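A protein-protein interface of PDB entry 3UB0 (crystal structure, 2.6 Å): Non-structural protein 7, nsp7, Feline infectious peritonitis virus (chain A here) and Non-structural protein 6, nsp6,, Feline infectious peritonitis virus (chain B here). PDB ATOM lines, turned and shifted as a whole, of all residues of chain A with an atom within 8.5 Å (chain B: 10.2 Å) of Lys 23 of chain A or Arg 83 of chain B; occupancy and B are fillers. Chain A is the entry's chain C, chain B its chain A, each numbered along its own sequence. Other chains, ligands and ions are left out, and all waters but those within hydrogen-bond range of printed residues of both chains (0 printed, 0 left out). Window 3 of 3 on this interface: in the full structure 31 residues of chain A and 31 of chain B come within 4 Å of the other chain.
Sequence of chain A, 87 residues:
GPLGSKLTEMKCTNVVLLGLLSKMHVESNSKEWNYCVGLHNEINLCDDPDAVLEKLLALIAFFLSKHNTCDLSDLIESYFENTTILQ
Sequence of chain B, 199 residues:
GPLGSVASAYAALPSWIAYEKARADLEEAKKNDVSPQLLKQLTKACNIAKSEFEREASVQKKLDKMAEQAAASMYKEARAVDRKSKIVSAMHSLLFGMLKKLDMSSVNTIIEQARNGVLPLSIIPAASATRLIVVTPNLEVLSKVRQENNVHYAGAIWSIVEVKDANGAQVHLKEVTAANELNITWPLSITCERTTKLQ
The side-chain amino group (NZ) of Lys 23 of chain A lies close to the backbone NH (N) of Arg 83 of chain B, 2.9 Å away.
Printed residues of chain B within 4 Å of Lys 23 of chain A: Arg 83, Val 88 and Met 91. Of chain A, only Lys 23 comes within 4 Å of Arg 83 of chain B. No residue of chain B comes within 4 Å of Ser 22 of chain A. Of the printed residues of chain A, Val 88 of chain B touches Leu 20 and Lys 23. Printed residues of chain A within 4 Å of His 92 of chain B: Leu 20 (3.9 Å) and Met 24 (3.97 Å). Of the printed residues of chain B, Leu 20 of chain A touches Val 88 (3.97 Å), Met 91 (3.7 Å) and His 92 (3.9 Å). The nearest printed residue of chain B that does not touch Lys 23 of chain A is Ile 87 of chain B (4.7 Å). The nearest residue of chain A that does not touch Arg 83 of chain B is His 25 of chain A (8.1 Å). The nearest printed residue of chain B that does not touch Leu 20 of chain A is Ile 87 of chain B (5.8 Å).
Printed residues of chain B that touch a printed residue of chain A: Arg 83, Val 88, Met 91 and His 92. Hydrophobic or aromatic side chains of chain A within 4 Å of the printed part of chain B: Val 16, Leu 20 and Met 24. Among the printed residues, 8 pairs touch across the chains.
O of Val 88 of chain B sits at hydrogen-bond distance from ND1 of His 92 of chain B.
O of Met 91 of chain B touches CG1 of Val 16 of chain A, at 3.6 Å. CD1 of Leu 20 of chain A touches O of Val 88 of chain B, at 3.97 Å. Met 91 of chain B touches Leu 20 of chain A. CD1 of Leu 20 of chain A touches CD2 of His 92 of chain B (3.9 Å). Lys 23 of chain A touches Val 88 of chain B (CD to CG2, 3.9997 Å). Lys 23 of chain A touches Met 91 of chain B (CG to CE, 3.7 Å). His 92 of chain B touches Met 24 of chain A (NE2 to CE, 3.97 Å).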
ATOM      1  N   VAL A  16      17.954  -6.333  27.507  1.00  0.00           N
ATOM      2  CA  VAL A  16      18.472  -5.297  26.593  1.00  0.00           C
ATOM      3  C   VAL A  16      17.374  -4.869  25.600  1.00  0.00           C
ATOM      4  O   VAL A  16      17.193  -3.669  25.385  1.00  0.00           O
ATOM      5  CB  VAL A  16      19.795  -5.693  25.894  1.00  0.00           C
ATOM      6  CG1 VAL A  16      20.309  -4.559  25.003  1.00  0.00           C
ATOM      7  CG2 VAL A  16      20.860  -6.099  26.908  1.00  0.00           C
ATOM      8  N   LEU A  17      16.609  -5.843  25.053  1.00  0.00           N
ATOM      9  CA  LEU A  17      15.489  -5.602  24.127  1.00  0.00           C
ATOM     10  C   LEU A  17      14.438  -4.704  24.765  1.00  0.00           C
ATOM     11  O   LEU A  17      14.051  -3.712  24.156  1.00  0.00           O
ATOM     12  CB  LEU A  17      14.822  -6.918  23.681  1.00  0.00           C
ATOM     13  CG  LEU A  17      15.425  -7.642  22.510  1.00  0.00           C
ATOM     14  CD1 LEU A  17      14.941  -9.051  22.479  1.00  0.00           C
ATOM     15  CD2 LEU A  17      15.125  -6.941  21.205  1.00  0.00           C
ATOM     16  N   LEU A  18      14.000  -5.019  25.994  1.00  0.00           N
ATOM     17  CA  LEU A  18      13.014  -4.190  26.680  1.00  0.00           C
ATOM     18  C   LEU A  18      13.515  -2.783  26.942  1.00  0.00           C
ATOM     19  O   LEU A  18      12.741  -1.840  26.796  1.00  0.00           O
ATOM     20  CB  LEU A  18      12.438  -4.835  27.953  1.00  0.00           C
ATOM     21  CG  LEU A  18      11.135  -4.167  28.458  1.00  0.00           C
ATOM     22  CD1 LEU A  18       9.911  -4.587  27.620  1.00  0.00           C
ATOM     23  CD2 LEU A  18      10.937  -4.379  29.942  1.00  0.00           C
ATOM     24  N   GLY A  19      14.792  -2.661  27.287  1.00  0.00           N
ATOM     25  CA  GLY A  19      15.457  -1.379  27.507  1.00  0.00           C
ATOM     26  C   GLY A  19      15.458  -0.536  26.245  1.00  0.00           C
ATOM     27  O   GLY A  19      15.079   0.634  26.282  1.00  0.00           O
ATOM     28  N   LEU A  20      15.815  -1.163  25.108  1.00  0.00           N
ATOM     29  CA  LEU A  20      15.794  -0.569  23.757  1.00  0.00           C
ATOM     30  C   LEU A  20      14.337  -0.150  23.397  1.00  0.00           C
ATOM     31  O   LEU A  20      14.104   1.009  23.048  1.00  0.00           O
ATOM     32  CB  LEU A  20      16.308  -1.610  22.750  1.00  0.00           C
ATOM     33  CG  LEU A  20      17.480  -1.343  21.794  1.00  0.00           C
ATOM     34  CD1 LEU A  20      18.153   0.005  21.995  1.00  0.00           C
ATOM     35  CD2 LEU A  20      18.452  -2.513  21.791  1.00  0.00           C
ATOM     36  N   LEU A  21      13.357  -1.066  23.554  1.00  0.00           N
ATOM     37  CA  LEU A  21      11.942  -0.777  23.254  1.00  0.00           C
ATOM     38  C   LEU A  21      11.359   0.419  24.020  1.00  0.00           C
ATOM     39  O   LEU A  21      10.650   1.222  23.436  1.00  0.00           O
ATOM     40  CB  LEU A  21      11.067  -2.027  23.388  1.00  0.00           C
ATOM     41  CG  LEU A  21      11.306  -3.117  22.303  1.00  0.00           C
ATOM     42  CD1 LEU A  21      10.943  -4.495  22.826  1.00  0.00           C
ATOM     43  CD2 LEU A  21      10.532  -2.816  21.009  1.00  0.00           C
ATOM     44  N   SER A  22      11.736   0.567  25.298  1.00  0.00           N
ATOM     45  CA  SER A  22      11.384   1.642  26.223  1.00  0.00           C
ATOM     46  C   SER A  22      11.887   3.000  25.705  1.00  0.00           C
ATOM     47  O   SER A  22      11.203   4.010  25.876  1.00  0.00           O
ATOM     48  CB  SER A  22      12.008   1.335  27.577  1.00  0.00           C
ATOM     49  OG  SER A  22      11.732   2.318  28.552  1.00  0.00           O
ATOM     50  N   LYS A  23      13.085   3.010  25.056  1.00  0.00           N
ATOM     51  CA  LYS A  23      13.727   4.196  24.466  1.00  0.00           C
ATOM     52  C   LYS A  23      13.091   4.522  23.113  1.00  0.00           C
ATOM     53  O   LYS A  23      13.341   5.578  22.571  1.00  0.00           O
ATOM     54  CB  LYS A  23      15.242   3.978  24.291  1.00  0.00           C
ATOM     55  CG  LYS A  23      15.999   3.841  25.595  1.00  0.00           C
ATOM     56  CD  LYS A  23      16.979   4.976  25.835  1.00  0.00           C
ATOM     57  CE  LYS A  23      16.351   6.186  26.494  1.00  0.00           C
ATOM     58  NZ  LYS A  23      15.934   7.210  25.492  1.00  0.00           N
ATOM     59  N   MET A  24      12.277   3.616  22.571  1.00  0.00           N
ATOM     60  CA  MET A  24      11.602   3.799  21.291  1.00  0.00           C
ATOM     61  C   MET A  24      10.196   4.326  21.483  1.00  0.00           C
ATOM     62  O   MET A  24       9.427   4.359  20.526  1.00  0.00           O
ATOM     63  CB  MET A  24      11.599   2.488  20.491  1.00  0.00           C
ATOM     64  CG  MET A  24      12.890   2.245  19.768  1.00  0.00           C
ATOM     65  SD  MET A  24      13.157   0.505  19.327  1.00  0.00           S
ATOM     66  CE  MET A  24      14.945   0.650  18.723  1.00  0.00           C
ATOM     67  N   HIS A  25       9.856   4.752  22.711  1.00  0.00           N
ATOM     68  CA  HIS A  25       8.543   5.296  23.061  1.00  0.00           C
ATOM     69  C   HIS A  25       7.330   4.438  22.611  1.00  0.00           C
ATOM     70  O   HIS A  25       6.389   4.947  22.005  1.00  0.00           O
ATOM     71  CB  HIS A  25       8.424   6.784  22.647  1.00  0.00           C
ATOM     72  CG  HIS A  25       9.378   7.690  23.369  1.00  0.00           C
ATOM     73  ND1 HIS A  25       9.457   7.707  24.763  1.00  0.00           N
ATOM     74  CD2 HIS A  25      10.247   8.604  22.872  1.00  0.00           C
ATOM     75  CE1 HIS A  25      10.377   8.612  25.059  1.00  0.00           C
ATOM     76  NE2 HIS A  25      10.875   9.184  23.958  1.00  0.00           N
ATOM     77  N   VAL A  26       7.358   3.139  22.937  1.00  0.00           N
ATOM     78  CA  VAL A  26       6.278   2.192  22.625  1.00  0.00           C
ATOM     79  C   VAL A  26       5.176   2.410  23.667  1.00  0.00           C
ATOM     80  O   VAL A  26       4.016   2.075  23.424  1.00  0.00           O
ATOM     81  CB  VAL A  26       6.825   0.727  22.576  1.00  0.00           C
ATOM     82  CG1 VAL A  26       5.713  -0.309  22.382  1.00  0.00           C
ATOM     83  CG2 VAL A  26       7.897   0.580  21.496  1.00  0.00           C
ATOM     84  N   GLU A  27       5.534   3.053  24.793  1.00  0.00           N
ATOM     85  CA  GLU A  27       4.630   3.382  25.889  1.00  0.00           C
ATOM     86  C   GLU A  27       3.374   4.147  25.453  1.00  0.00           C
ATOM     87  O   GLU A  27       2.338   4.009  26.107  1.00  0.00           O
ATOM     88  CB  GLU A  27       5.380   4.120  27.002  1.00  0.00           C
ATOM     89  CG  GLU A  27       6.204   3.181  27.861  1.00  0.00           C
ATOM     90  CD  GLU A  27       6.786   3.780  29.125  1.00  0.00           C
ATOM     91  OE1 GLU A  27       8.032   3.768  29.254  1.00  0.00           O
ATOM     92  OE2 GLU A  27       6.003   4.209  30.006  1.00  0.00           O
ATOM     93  N   TRP A  33       2.669  -1.843  24.382  1.00  0.00           N
ATOM     94  CA  TRP A  33       3.520  -1.821  25.558  1.00  0.00           C
ATOM     95  C   TRP A  33       3.280  -2.988  26.496  1.00  0.00           C
ATOM     96  O   TRP A  33       4.236  -3.607  26.937  1.00  0.00           O
ATOM     97  CB  TRP A  33       3.456  -0.485  26.300  1.00  0.00           C
ATOM     98  CG  TRP A  33       4.571  -0.329  27.299  1.00  0.00           C
ATOM     99  CD1 TRP A  33       4.446  -0.073  28.633  1.00  0.00           C
ATOM    100  CD2 TRP A  33       5.982  -0.512  27.053  1.00  0.00           C
ATOM    101  NE1 TRP A  33       5.690  -0.041  29.227  1.00  0.00           N
ATOM    102  CE2 TRP A  33       6.651  -0.303  28.278  1.00  0.00           C
ATOM    103  CE3 TRP A  33       6.749  -0.790  25.904  1.00  0.00           C
ATOM    104  CZ2 TRP A  33       8.046  -0.397  28.396  1.00  0.00           C
ATOM    105  CZ3 TRP A  33       8.126  -0.884  26.023  1.00  0.00           C
ATOM    106  CH2 TRP A  33       8.763  -0.686  27.254  1.00  0.00           C
ATOM    107  N   MET B  74      18.657  13.370  40.508  1.00  0.00           N
ATOM    108  CA  MET B  74      18.013  12.890  39.276  1.00  0.00           C
ATOM    109  C   MET B  74      17.511  14.061  38.437  1.00  0.00           C
ATOM    110  O   MET B  74      17.664  14.049  37.217  1.00  0.00           O
ATOM    111  CB  MET B  74      16.862  11.917  39.558  1.00  0.00           C
ATOM    112  CG  MET B  74      16.326  11.268  38.284  1.00  0.00           C
ATOM    113  SD  MET B  74      14.557  10.480  38.433  1.00  0.00           S
ATOM    114  CE  MET B  74      14.091  10.485  36.550  1.00  0.00           C
ATOM    115  N   LYS B  76      18.574  16.648  37.554  1.00  0.00           N
ATOM    116  CA  LYS B  76      19.602  16.986  36.556  1.00  0.00           C
ATOM    117  C   LYS B  76      19.175  16.583  35.131  1.00  0.00           C
ATOM    118  O   LYS B  76      19.369  17.373  34.203  1.00  0.00           O
ATOM    119  CB  LYS B  76      20.934  16.294  36.908  1.00  0.00           C
ATOM    120  CG  LYS B  76      21.794  17.043  37.928  1.00  0.00           C
ATOM    121  CD  LYS B  76      22.720  18.102  37.284  1.00  0.00           C
ATOM    122  CE  LYS B  76      23.965  17.549  36.611  1.00  0.00           C
ATOM    123  NZ  LYS B  76      23.808  17.455  35.135  1.00  0.00           N
ATOM    124  N   GLU B  77      18.583  15.363  34.972  1.00  0.00           N
ATOM    125  CA  GLU B  77      18.073  14.797  33.714  1.00  0.00           C
ATOM    126  C   GLU B  77      17.077  15.722  32.995  1.00  0.00           C
ATOM    127  O   GLU B  77      16.212  16.329  33.626  1.00  0.00           O
ATOM    128  CB  GLU B  77      17.417  13.435  33.966  1.00  0.00           C
ATOM    129  CG  GLU B  77      18.303  12.261  33.612  1.00  0.00           C
ATOM    130  CD  GLU B  77      17.689  10.917  33.947  1.00  0.00           C
ATOM    131  OE1 GLU B  77      16.924  10.379  33.113  1.00  0.00           O
ATOM    132  OE2 GLU B  77      17.977  10.399  35.051  1.00  0.00           O
ATOM    133  N   ARG B  83      18.726   8.023  25.683  1.00  0.00           N
ATOM    134  CA  ARG B  83      19.157   9.321  26.185  1.00  0.00           C
ATOM    135  C   ARG B  83      20.044   9.922  25.074  1.00  0.00           C
ATOM    136  O   ARG B  83      19.630  10.796  24.280  1.00  0.00           O
ATOM    137  CB  ARG B  83      19.931   9.132  27.508  1.00  0.00           C
ATOM    138  CG  ARG B  83      20.019  10.370  28.392  1.00  0.00           C
ATOM    139  CD  ARG B  83      21.409  10.606  28.976  1.00  0.00           C
ATOM    140  NE  ARG B  83      22.318  11.260  28.026  1.00  0.00           N
ATOM    141  CZ  ARG B  83      22.358  12.573  27.783  1.00  0.00           C
ATOM    142  NH1 ARG B  83      23.221  13.065  26.905  1.00  0.00           N
ATOM    143  NH2 ARG B  83      21.527  13.401  28.411  1.00  0.00           N
ATOM    144  N   LYS B  84      21.246   9.370  24.984  1.00  0.00           N
ATOM    145  CA  LYS B  84      22.221   9.682  23.969  1.00  0.00           C
ATOM    146  C   LYS B  84      21.866   8.835  22.730  1.00  0.00           C
ATOM    147  O   LYS B  84      21.212   7.783  22.855  1.00  0.00           O
ATOM    148  CB  LYS B  84      23.615   9.256  24.488  1.00  0.00           C
ATOM    149  CG  LYS B  84      24.261  10.198  25.491  1.00  0.00           C
ATOM    150  CD  LYS B  84      25.589   9.642  26.005  1.00  0.00           C
ATOM    151  CE  LYS B  84      26.307  10.630  26.898  1.00  0.00           C
ATOM    152  NZ  LYS B  84      27.453  11.290  26.210  1.00  0.00           N
ATOM    153  N   SER B  85      22.326   9.277  21.531  1.00  0.00           N
ATOM    154  CA  SER B  85      22.265   8.455  20.326  1.00  0.00           C
ATOM    155  C   SER B  85      23.265   7.331  20.734  1.00  0.00           C
ATOM    156  O   SER B  85      22.952   6.158  20.556  1.00  0.00           O
ATOM    157  CB  SER B  85      22.771   9.226  19.109  1.00  0.00           C
ATOM    158  OG  SER B  85      22.494   8.524  17.907  1.00  0.00           O
ATOM    159  N   LYS B  86      24.380   7.732  21.451  1.00  0.00           N
ATOM    160  CA  LYS B  86      25.427   6.909  22.077  1.00  0.00           C
ATOM    161  C   LYS B  86      24.873   5.817  23.016  1.00  0.00           C
ATOM    162  O   LYS B  86      25.307   4.676  22.842  1.00  0.00           O
ATOM    163  CB  LYS B  86      26.452   7.779  22.822  1.00  0.00           C
ATOM    164  CG  LYS B  86      27.769   7.933  22.101  1.00  0.00           C
ATOM    165  CD  LYS B  86      28.875   7.107  22.738  1.00  0.00           C
ATOM    166  CE  LYS B  86      30.032   7.981  23.164  1.00  0.00           C
ATOM    167  NZ  LYS B  86      31.206   7.187  23.619  1.00  0.00           N
ATOM    168  N   ILE B  87      23.935   6.142  23.990  1.00  0.00           N
ATOM    169  CA  ILE B  87      23.302   5.131  24.877  1.00  0.00           C
ATOM    170  C   ILE B  87      22.491   4.097  24.065  1.00  0.00           C
ATOM    171  O   ILE B  87      22.605   2.902  24.303  1.00  0.00           O
ATOM    172  CB  ILE B  87      22.498   5.747  26.065  1.00  0.00           C
ATOM    173  CG1 ILE B  87      23.473   6.321  27.116  1.00  0.00           C
ATOM    174  CG2 ILE B  87      21.546   4.720  26.750  1.00  0.00           C
ATOM    175  CD1 ILE B  87      22.984   7.549  27.824  1.00  0.00           C
ATOM    176  N   VAL B  88      21.717   4.563  23.088  1.00  0.00           N
ATOM    177  CA  VAL B  88      20.937   3.705  22.206  1.00  0.00           C
ATOM    178  C   VAL B  88      21.897   2.853  21.352  1.00  0.00           C
ATOM    179  O   VAL B  88      21.674   1.651  21.199  1.00  0.00           O
ATOM    180  CB  VAL B  88      19.908   4.529  21.383  1.00  0.00           C
ATOM    181  CG1 VAL B  88      19.281   3.708  20.268  1.00  0.00           C
ATOM    182  CG2 VAL B  88      18.834   5.110  22.294  1.00  0.00           C
ATOM    183  N   SER B  89      23.007   3.469  20.881  1.00  0.00           N
ATOM    184  CA  SER B  89      24.050   2.808  20.095  1.00  0.00           C
ATOM    185  C   SER B  89      24.765   1.712  20.901  1.00  0.00           C
ATOM    186  O   SER B  89      25.051   0.642  20.350  1.00  0.00           O
ATOM    187  CB  SER B  89      25.056   3.822  19.571  1.00  0.00           C
ATOM    188  OG  SER B  89      24.429   4.624  18.590  1.00  0.00           O
ATOM    189  N   ALA B  90      25.005   1.969  22.203  1.00  0.00           N
ATOM    190  CA  ALA B  90      25.659   1.037  23.113  1.00  0.00           C
ATOM    191  C   ALA B  90      24.776  -0.188  23.340  1.00  0.00           C
ATOM    192  O   ALA B  90      25.288  -1.320  23.362  1.00  0.00           O
ATOM    193  CB  ALA B  90      25.987   1.730  24.428  1.00  0.00           C
ATOM    194  N   MET B  91      23.450   0.032  23.469  1.00  0.00           N
ATOM    195  CA  MET B  91      22.469  -1.052  23.614  1.00  0.00           C
ATOM    196  C   MET B  91      22.337  -1.827  22.305  1.00  0.00           C
ATOM    197  O   MET B  91      22.189  -3.047  22.354  1.00  0.00           O
ATOM    198  CB  MET B  91      21.107  -0.550  24.067  1.00  0.00           C
ATOM    199  CG  MET B  91      21.126   0.162  25.413  1.00  0.00           C
ATOM    200  SD  MET B  91      19.365   0.836  26.009  1.00  0.00           S
ATOM    201  CE  MET B  91      19.185   2.197  24.775  1.00  0.00           C
ATOM    202  N   HIS B  92      22.412  -1.137  21.141  1.00  0.00           N
ATOM    203  CA  HIS B  92      22.335  -1.809  19.838  1.00  0.00           C
ATOM    204  C   HIS B  92      23.539  -2.737  19.647  1.00  0.00           C
ATOM    205  O   HIS B  92      23.380  -3.873  19.197  1.00  0.00           O
ATOM    206  CB  HIS B  92      22.286  -0.815  18.664  1.00  0.00           C
ATOM    207  CG  HIS B  92      20.951  -0.200  18.350  1.00  0.00           C
ATOM    208  ND1 HIS B  92      20.891   1.096  17.903  1.00  0.00           N
ATOM    209  CD2 HIS B  92      19.691  -0.673  18.467  1.00  0.00           C
ATOM    210  CE1 HIS B  92      19.616   1.376  17.750  1.00  0.00           C
ATOM    211  NE2 HIS B  92      18.851   0.358  18.087  1.00  0.00           N
